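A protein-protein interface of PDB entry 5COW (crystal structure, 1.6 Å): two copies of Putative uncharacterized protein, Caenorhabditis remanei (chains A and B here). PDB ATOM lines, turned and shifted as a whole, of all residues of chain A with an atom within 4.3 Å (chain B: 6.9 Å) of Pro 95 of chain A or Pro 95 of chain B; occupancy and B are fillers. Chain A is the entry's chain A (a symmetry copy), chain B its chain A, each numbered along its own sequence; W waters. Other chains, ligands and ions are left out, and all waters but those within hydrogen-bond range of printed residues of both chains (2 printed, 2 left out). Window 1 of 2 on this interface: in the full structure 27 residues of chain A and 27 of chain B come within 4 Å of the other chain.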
ATOM      1  N   LEU A  91       0.827 -25.861  13.829  1.00  0.00           N
ATOM      2  CA  LEU A  91       0.717 -25.119  12.569  1.00  0.00           C
ATOM      3  C   LEU A  91      -0.690 -24.595  12.295  1.00  0.00           C
ATOM      4  O   LEU A  91      -0.853 -23.577  11.612  1.00  0.00           O
ATOM      5  CB  LEU A  91       1.154 -25.996  11.395  1.00  0.00           C
ATOM      6  CG  LEU A  91       2.643 -26.310  11.286  1.00  0.00           C
ATOM      7  CD1 LEU A  91       2.883 -27.186  10.062  1.00  0.00           C
ATOM      8  CD2 LEU A  91       3.461 -25.027  11.221  1.00  0.00           C
ATOM      9  N   GLU A  92      -1.704 -25.297  12.803  1.00  0.00           N
ATOM     10  CA  GLU A  92      -3.097 -24.882  12.638  1.00  0.00           C
ATOM     11  C   GLU A  92      -3.630 -24.000  13.788  1.00  0.00           C
ATOM     12  O   GLU A  92      -4.448 -23.113  13.557  1.00  0.00           O
ATOM     13  CB  GLU A  92      -4.004 -26.107  12.492  1.00  0.00           C
ATOM     14  CG  GLU A  92      -3.592 -27.037  11.352  1.00  0.00           C
ATOM     15  CD  GLU A  92      -4.669 -28.047  10.982  1.00  0.00           C
ATOM     16  OE1 GLU A  92      -5.756 -28.040  11.605  1.00  0.00           O
ATOM     17  OE2 GLU A  92      -4.422 -28.842  10.049  1.00  0.00           O
ATOM     18  N   VAL A  93      -3.161 -24.246  15.009  1.00  0.00           N
ATOM     19  CA  VAL A  93      -3.640 -23.522  16.191  1.00  0.00           C
ATOM     20  C   VAL A  93      -2.973 -22.154  16.313  1.00  0.00           C
ATOM     21  O   VAL A  93      -3.597 -21.191  16.793  1.00  0.00           O
ATOM     22  CB  VAL A  93      -3.410 -24.352  17.477  1.00  0.00           C
ATOM     23  CG1 VAL A  93      -3.847 -23.577  18.735  1.00  0.00           C
ATOM     24  CG2 VAL A  93      -4.176 -25.667  17.386  1.00  0.00           C
ATOM     25  N   PHE A  94      -1.720 -22.060  15.870  1.00  0.00           N
ATOM     26  CA  PHE A  94      -0.991 -20.784  15.871  1.00  0.00           C
ATOM     27  C   PHE A  94      -0.563 -20.457  14.431  1.00  0.00           C
ATOM     28  O   PHE A  94       0.620 -20.511  14.111  1.00  0.00           O
ATOM     29  CB  PHE A  94       0.256 -20.832  16.777  1.00  0.00           C
ATOM     30  CG  PHE A  94       0.003 -21.343  18.176  1.00  0.00           C
ATOM     31  CD1 PHE A  94       0.090 -22.696  18.462  1.00  0.00           C
ATOM     32  CD2 PHE A  94      -0.290 -20.466  19.211  1.00  0.00           C
ATOM     33  CE1 PHE A  94      -0.132 -23.170  19.748  1.00  0.00           C
ATOM     34  CE2 PHE A  94      -0.509 -20.935  20.506  1.00  0.00           C
ATOM     35  CZ  PHE A  94      -0.433 -22.286  20.773  1.00  0.00           C
ATOM     36  N   PRO A  95      -1.528 -20.131  13.559  1.00  0.00           N
ATOM     37  CA  PRO A  95      -1.201 -20.010  12.128  1.00  0.00           C
ATOM     38  C   PRO A  95      -0.251 -18.857  11.783  1.00  0.00           C
ATOM     39  O   PRO A  95      -0.328 -17.769  12.366  1.00  0.00           O
ATOM     40  CB  PRO A  95      -2.569 -19.789  11.476  1.00  0.00           C
ATOM     41  CG  PRO A  95      -3.433 -19.259  12.573  1.00  0.00           C
ATOM     42  CD  PRO A  95      -2.964 -19.947  13.815  1.00  0.00           C
ATOM     43  N   GLY A  96       0.658 -19.116  10.846  1.00  0.00           N
ATOM     44  CA  GLY A  96       1.571 -18.096  10.364  1.00  0.00           C
ATOM     45  C   GLY A  96       2.375 -17.415  11.452  1.00  0.00           C
ATOM     46  O   GLY A  96       3.012 -18.067  12.279  1.00  0.00           O
ATOM     47  N   LEU A  97       2.309 -16.087  11.464  1.00  0.00           N
ATOM     48  CA  LEU A  97       3.118 -15.284  12.361  1.00  0.00           C
ATOM     49  C   LEU A  97       2.686 -15.424  13.822  1.00  0.00           C
ATOM     50  O   LEU A  97       3.420 -15.025  14.733  1.00  0.00           O
ATOM     51  CB  LEU A  97       3.051 -13.819  11.914  1.00  0.00           C
ATOM     52  CG  LEU A  97       4.047 -12.805  12.462  1.00  0.00           C
ATOM     53  CD1 LEU A  97       5.486 -13.247  12.255  1.00  0.00           C
ATOM     54  CD2 LEU A  97       3.787 -11.459  11.780  1.00  0.00           C
ATOM     55  N   GLN A  98       1.496 -15.979  14.054  1.00  0.00           N
ATOM     56  CA  GLN A  98       1.047 -16.164  15.437  1.00  0.00           C
ATOM     57  C   GLN A  98       1.997 -17.059  16.233  1.00  0.00           C
ATOM     58  O   GLN A  98       2.156 -16.886  17.439  1.00  0.00           O
ATOM     59  CB  GLN A  98      -0.370 -16.729  15.477  1.00  0.00           C
ATOM     60  CG  GLN A  98      -1.408 -15.729  15.026  1.00  0.00           C
ATOM     61  CD  GLN A  98      -2.824 -16.275  15.057  1.00  0.00           C
ATOM     62  OE1 GLN A  98      -3.130 -17.203  15.808  1.00  0.00           O
ATOM     63  NE2 GLN A  98      -3.697 -15.686  14.256  1.00  0.00           N
ATOM     64  N   LYS A 150      -8.221 -14.147  20.442  1.00  0.00           N
ATOM     65  CA  LYS A 150      -8.456 -15.568  20.713  1.00  0.00           C
ATOM     66  C   LYS A 150      -8.476 -15.882  22.214  1.00  0.00           C
ATOM     67  O   LYS A 150      -9.294 -16.694  22.660  1.00  0.00           O
ATOM     68  CB  LYS A 150      -7.408 -16.437  20.004  1.00  0.00           C
ATOM     69  CG  LYS A 150      -7.627 -16.549  18.493  1.00  0.00           C
ATOM     70  CD  LYS A 150      -6.521 -17.391  17.849  1.00  0.00           C
ATOM     71  CE  LYS A 150      -6.812 -17.659  16.388  1.00  0.00           C
ATOM     72  NZ  LYS A 150      -5.722 -18.474  15.765  1.00  0.00           N
ATOM     73  N   LEU B  52       7.935 -15.525   7.703  1.00  0.00           N
ATOM     74  CA  LEU B  52       6.580 -15.438   8.237  1.00  0.00           C
ATOM     75  C   LEU B  52       6.049 -14.008   8.177  1.00  0.00           C
ATOM     76  O   LEU B  52       4.862 -13.786   7.907  1.00  0.00           O
ATOM     77  CB  LEU B  52       6.529 -15.944   9.676  1.00  0.00           C
ATOM     78  CG  LEU B  52       6.765 -17.443   9.866  1.00  0.00           C
ATOM     79  CD1 LEU B  52       6.791 -17.763  11.349  1.00  0.00           C
ATOM     80  CD2 LEU B  52       5.682 -18.236   9.168  1.00  0.00           C
ATOM     81  N   PHE B  63      -6.096  -9.590   0.833  1.00  0.00           N
ATOM     82  CA  PHE B  63      -7.346  -9.091   1.412  1.00  0.00           C
ATOM     83  C   PHE B  63      -7.633  -7.653   1.017  1.00  0.00           C
ATOM     84  O   PHE B  63      -8.802  -7.267   0.975  1.00  0.00           O
ATOM     85  CB  PHE B  63      -7.340  -9.275   2.940  1.00  0.00           C
ATOM     86  CG  PHE B  63      -7.517 -10.711   3.344  1.00  0.00           C
ATOM     87  CD1 PHE B  63      -8.712 -11.374   3.070  1.00  0.00           C
ATOM     88  CD2 PHE B  63      -6.474 -11.422   3.925  1.00  0.00           C
ATOM     89  CE1 PHE B  63      -8.872 -12.714   3.400  1.00  0.00           C
ATOM     90  CE2 PHE B  63      -6.627 -12.761   4.256  1.00  0.00           C
ATOM     91  CZ  PHE B  63      -7.818 -13.408   3.997  1.00  0.00           C
ATOM     92  N   ARG B  90      -3.342 -20.963  -0.093  1.00  0.00           N
ATOM     93  CA  ARG B  90      -4.702 -20.820   0.432  1.00  0.00           C
ATOM     94  C   ARG B  90      -4.792 -21.352   1.860  1.00  0.00           C
ATOM     95  O   ARG B  90      -5.485 -20.781   2.712  1.00  0.00           O
ATOM     96  CB  ARG B  90      -5.686 -21.569  -0.476  1.00  0.00           C
ATOM     97  CG  ARG B  90      -7.047 -20.941  -0.662  1.00  0.00           C
ATOM     98  CD  ARG B  90      -7.662 -21.396  -1.999  1.00  0.00           C
ATOM     99  NE  ARG B  90      -7.755 -22.845  -2.110  1.00  0.00           N
ATOM    100  CZ  ARG B  90      -7.639 -23.530  -3.248  1.00  0.00           C
ATOM    101  NH1 ARG B  90      -7.411 -22.906  -4.399  1.00  0.00           N
ATOM    102  NH2 ARG B  90      -7.740 -24.851  -3.233  1.00  0.00           N
ATOM    103  N   LEU B  91      -4.085 -22.445   2.122  1.00  0.00           N
ATOM    104  CA  LEU B  91      -4.068 -23.027   3.469  1.00  0.00           C
ATOM    105  C   LEU B  91      -3.518 -22.080   4.531  1.00  0.00           C
ATOM    106  O   LEU B  91      -3.889 -22.179   5.707  1.00  0.00           O
ATOM    107  CB  LEU B  91      -3.245 -24.315   3.482  1.00  0.00           C
ATOM    108  CG  LEU B  91      -3.846 -25.525   2.774  1.00  0.00           C
ATOM    109  CD1 LEU B  91      -2.889 -26.705   2.897  1.00  0.00           C
ATOM    110  CD2 LEU B  91      -5.216 -25.859   3.348  1.00  0.00           C
ATOM    111  N   GLU B  92      -2.619 -21.180   4.130  1.00  0.00           N
ATOM    112  CA  GLU B  92      -2.040 -20.195   5.044  1.00  0.00           C
ATOM    113  C   GLU B  92      -2.802 -18.853   5.087  1.00  0.00           C
ATOM    114  O   GLU B  92      -2.872 -18.217   6.135  1.00  0.00           O
ATOM    115  CB  GLU B  92      -0.579 -19.924   4.680  1.00  0.00           C
ATOM    116  CG  GLU B  92       0.285 -21.184   4.646  1.00  0.00           C
ATOM    117  CD  GLU B  92       1.778 -20.889   4.632  1.00  0.00           C
ATOM    118  OE1 GLU B  92       2.168 -19.699   4.651  1.00  0.00           O
ATOM    119  OE2 GLU B  92       2.561 -21.864   4.616  1.00  0.00           O
ATOM    120  N   VAL B  93      -3.369 -18.442   3.955  1.00  0.00           N
ATOM    121  CA  VAL B  93      -4.061 -17.153   3.852  1.00  0.00           C
ATOM    122  C   VAL B  93      -5.477 -17.236   4.419  1.00  0.00           C
ATOM    123  O   VAL B  93      -5.987 -16.251   4.983  1.00  0.00           O
ATOM    124  CB  VAL B  93      -4.095 -16.661   2.385  1.00  0.00           C
ATOM    125  CG1 VAL B  93      -4.878 -15.340   2.250  1.00  0.00           C
ATOM    126  CG2 VAL B  93      -2.672 -16.474   1.871  1.00  0.00           C
ATOM    127  N   PHE B  94      -6.104 -18.404   4.287  1.00  0.00           N
ATOM    128  CA  PHE B  94      -7.444 -18.632   4.847  1.00  0.00           C
ATOM    129  C   PHE B  94      -7.374 -19.812   5.829  1.00  0.00           C
ATOM    130  O   PHE B  94      -7.903 -20.883   5.547  1.00  0.00           O
ATOM    131  CB  PHE B  94      -8.484 -18.938   3.751  1.00  0.00           C
ATOM    132  CG  PHE B  94      -8.507 -17.952   2.607  1.00  0.00           C
ATOM    133  CD1 PHE B  94      -7.700 -18.137   1.496  1.00  0.00           C
ATOM    134  CD2 PHE B  94      -9.362 -16.858   2.628  1.00  0.00           C
ATOM    135  CE1 PHE B  94      -7.725 -17.239   0.437  1.00  0.00           C
ATOM    136  CE2 PHE B  94      -9.396 -15.956   1.566  1.00  0.00           C
ATOM    137  CZ  PHE B  94      -8.575 -16.145   0.473  1.00  0.00           C
ATOM    138  N   PRO B  95      -6.710 -19.621   6.979  1.00  0.00           N
ATOM    139  CA  PRO B  95      -6.439 -20.771   7.858  1.00  0.00           C
ATOM    140  C   PRO B  95      -7.686 -21.413   8.476  1.00  0.00           C
ATOM    141  O   PRO B  95      -8.643 -20.725   8.846  1.00  0.00           O
ATOM    142  CB  PRO B  95      -5.549 -20.170   8.951  1.00  0.00           C
ATOM    143  CG  PRO B  95      -5.846 -18.707   8.922  1.00  0.00           C
ATOM    144  CD  PRO B  95      -6.103 -18.382   7.485  1.00  0.00           C
ATOM    145  N   GLY B  96      -7.671 -22.742   8.563  1.00  0.00           N
ATOM    146  CA  GLY B  96      -8.748 -23.479   9.197  1.00  0.00           C
ATOM    147  C   GLY B  96     -10.122 -23.180   8.634  1.00  0.00           C
ATOM    148  O   GLY B  96     -10.344 -23.241   7.425  1.00  0.00           O
ATOM    149  N   LEU B  97     -11.039 -22.821   9.526  1.00  0.00           N
ATOM    150  CA  LEU B  97     -12.430 -22.624   9.165  1.00  0.00           C
ATOM    151  C   LEU B  97     -12.639 -21.384   8.294  1.00  0.00           C
ATOM    152  O   LEU B  97     -13.703 -21.217   7.686  1.00  0.00           O
ATOM    153  CB  LEU B  97     -13.269 -22.534  10.445  1.00  0.00           C
ATOM    154  CG  LEU B  97     -14.786 -22.653  10.378  1.00  0.00           C
ATOM    155  CD1 LEU B  97     -15.229 -23.922   9.667  1.00  0.00           C
ATOM    156  CD2 LEU B  97     -15.335 -22.607  11.805  1.00  0.00           C
ATOM    157  N   GLN B  98     -11.637 -20.506   8.235  1.00  0.00           N
ATOM    158  CA  GLN B  98     -11.773 -19.316   7.391  1.00  0.00           C
ATOM    159  C   GLN B  98     -11.991 -19.677   5.922  1.00  0.00           C
ATOM    160  O   GLN B  98     -12.671 -18.956   5.195  1.00  0.00           O
ATOM    161  CB  GLN B  98     -10.558 -18.404   7.537  1.00  0.00           C
ATOM    162  CG  GLN B  98     -10.496 -17.729   8.886  1.00  0.00           C
ATOM    163  CD  GLN B  98      -9.291 -16.820   9.050  1.00  0.00           C
ATOM    164  OE1 GLN B  98      -8.736 -16.319   8.070  1.00  0.00           O
ATOM    165  NE2 GLN B  98      -8.896 -16.588  10.291  1.00  0.00           N
ATOM    166  N   ARG B  99     -11.433 -20.800   5.479  1.00  0.00           N
ATOM    167  CA  ARG B  99     -11.665 -21.253   4.110  1.00  0.00           C
ATOM    168  C   ARG B  99     -13.151 -21.502   3.849  1.00  0.00           C
ATOM    169  O   ARG B  99     -13.692 -21.093   2.827  1.00  0.00           O
ATOM    170  CB  ARG B  99     -10.858 -22.527   3.832  1.00  0.00           C
ATOM    171  CG  ARG B  99     -11.175 -23.197   2.503  1.00  0.00           C
ATOM    172  CD  ARG B  99     -11.220 -24.717   2.651  1.00  0.00           C
ATOM    173  NE  ARG B  99     -10.105 -25.216   3.454  1.00  0.00           N
ATOM    174  CZ  ARG B  99      -9.925 -26.491   3.785  1.00  0.00           C
ATOM    175  NH1 ARG B  99     -10.789 -27.415   3.380  1.00  0.00           N
ATOM    176  NH2 ARG B  99      -8.882 -26.842   4.526  1.00  0.00           N
ATOM    177  N   SER B 100     -13.810 -22.142   4.809  1.00  0.00           N
ATOM    178  CA  SER B 100     -15.208 -22.532   4.688  1.00  0.00           C
ATOM    179  C   SER B 100     -16.170 -21.347   4.702  1.00  0.00           C
ATOM    180  O   SER B 100     -17.215 -21.378   4.051  1.00  0.00           O
ATOM    181  CB  SER B 100     -15.585 -23.490   5.826  1.00  0.00           C
ATOM    182  OG  SER B 100     -14.789 -24.661   5.794  1.00  0.00           O
ATOM    183  N   ALA B 143     -14.955 -17.304  12.933  1.00  0.00           N
ATOM    184  CA  ALA B 143     -14.145 -17.290  11.714  1.00  0.00           C
ATOM    185  C   ALA B 143     -14.570 -16.159  10.773  1.00  0.00           C
ATOM    186  O   ALA B 143     -13.721 -15.507  10.153  1.00  0.00           O
ATOM    187  CB  ALA B 143     -14.228 -18.645  10.998  1.00  0.00           C
ATOM    188  N   GLU B 146     -13.096 -13.051  12.185  1.00  0.00           N
ATOM    189  CA  GLU B 146     -11.667 -12.976  11.875  1.00  0.00           C
ATOM    190  C   GLU B 146     -11.437 -12.445  10.446  1.00  0.00           C
ATOM    191  O   GLU B 146     -10.528 -11.639  10.213  1.00  0.00           O
ATOM    192  CB  GLU B 146     -11.005 -14.351  12.062  1.00  0.00           C
ATOM    193  CG  GLU B 146     -10.921 -14.787  13.528  1.00  0.00           C
ATOM    194  CD  GLU B 146     -10.562 -16.258  13.701  1.00  0.00           C
ATOM    195  OE1 GLU B 146     -10.448 -16.981  12.686  1.00  0.00           O
ATOM    196  OE2 GLU B 146     -10.415 -16.695  14.863  1.00  0.00           O
ATOM    197  N   LEU B 147     -12.259 -12.892   9.496  1.00  0.00           N
ATOM    198  CA  LEU B 147     -12.109 -12.451   8.114  1.00  0.00           C
ATOM    199  C   LEU B 147     -12.560 -10.995   7.939  1.00  0.00           C
ATOM    200  O   LEU B 147     -11.897 -10.236   7.229  1.00  0.00           O
ATOM    201  CB  LEU B 147     -12.883 -13.371   7.163  1.00  0.00           C
ATOM    202  CG  LEU B 147     -12.206 -14.715   6.870  1.00  0.00           C
ATOM    203  CD1 LEU B 147     -13.167 -15.573   6.095  1.00  0.00           C
ATOM    204  CD2 LEU B 147     -10.944 -14.521   6.057  1.00  0.00           C
ATOM    205  N   LYS B 150      -9.735  -8.917   9.042  1.00  0.00           N
ATOM    206  CA  LYS B 150      -8.684  -8.896   8.020  1.00  0.00           C
ATOM    207  C   LYS B 150      -9.024  -7.965   6.850  1.00  0.00           C
ATOM    208  O   LYS B 150      -8.137  -7.271   6.340  1.00  0.00           O
ATOM    209  CB  LYS B 150      -8.401 -10.314   7.503  1.00  0.00           C
ATOM    210  CG  LYS B 150      -7.613 -11.178   8.490  1.00  0.00           C
ATOM    211  CD  LYS B 150      -7.408 -12.589   7.928  1.00  0.00           C
ATOM    212  CE  LYS B 150      -6.485 -13.405   8.807  1.00  0.00           C
ATOM    213  NZ  LYS B 150      -6.298 -14.783   8.254  1.00  0.00           N
HETATM  214  O   HOH W   1       2.755 -15.589   8.118  1.00  0.00           O
HETATM  215  O   HOH W   2      -2.493 -22.669   8.772  1.00  0.00           O
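Of chain B, only Pro 95 comes within 4 Å of Pro 95 of chain A.
Of the printed residues of chain B, Gly 96 of chain A touches Leu 52.
Of the printed residues of chain B, Leu 97 of chain A touches Leu 52.
Pro 95 of chain B touches just one residue of chain A: Pro 95 (3.9 Å).
Ser 100 of chain B touches none of the printed residues of chain A.
The nearest residue of chain B that does not touch Pro 95 of chain A is Glu 92 of chain B (5.6 Å).
Water W1 bridges O of Leu 52 of chain B (2.8 Å) and N of Leu 97 of chain A (3.4 Å).
Water W2 bridges the backbone carbonyl oxygen (O) of Leu 91 of chain A (3.4 Å) and the backbone carbonyl oxygen (O) of Leu 91 of chain B (3.4 Å).
Pro 95 of chain A touches its own counterpart, Pro 95 of chain B.
Pro 95 of chain A touches Pro 95 of chain B (CB to CB, 3.9 Å).
O of Gly 96 of chain A touches CD1 of Leu 52 of chain B, 3.9 Å away.
Leu 52 of chain B touches Leu 97 of chain A.
Hydrophobic or aromatic side chains of chain A within 4 Å of the printed part of chain B: Pro 95 and Leu 97.
Hydrophobic or aromatic side chains of chain B within 4 Å of the printed part of chain A: Leu 52 and Pro 95.
Along chain B the printed residues that touch a printed residue of chain A span positions 52 to 95.
Among the printed residues, 3 pairs touch across the chains.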
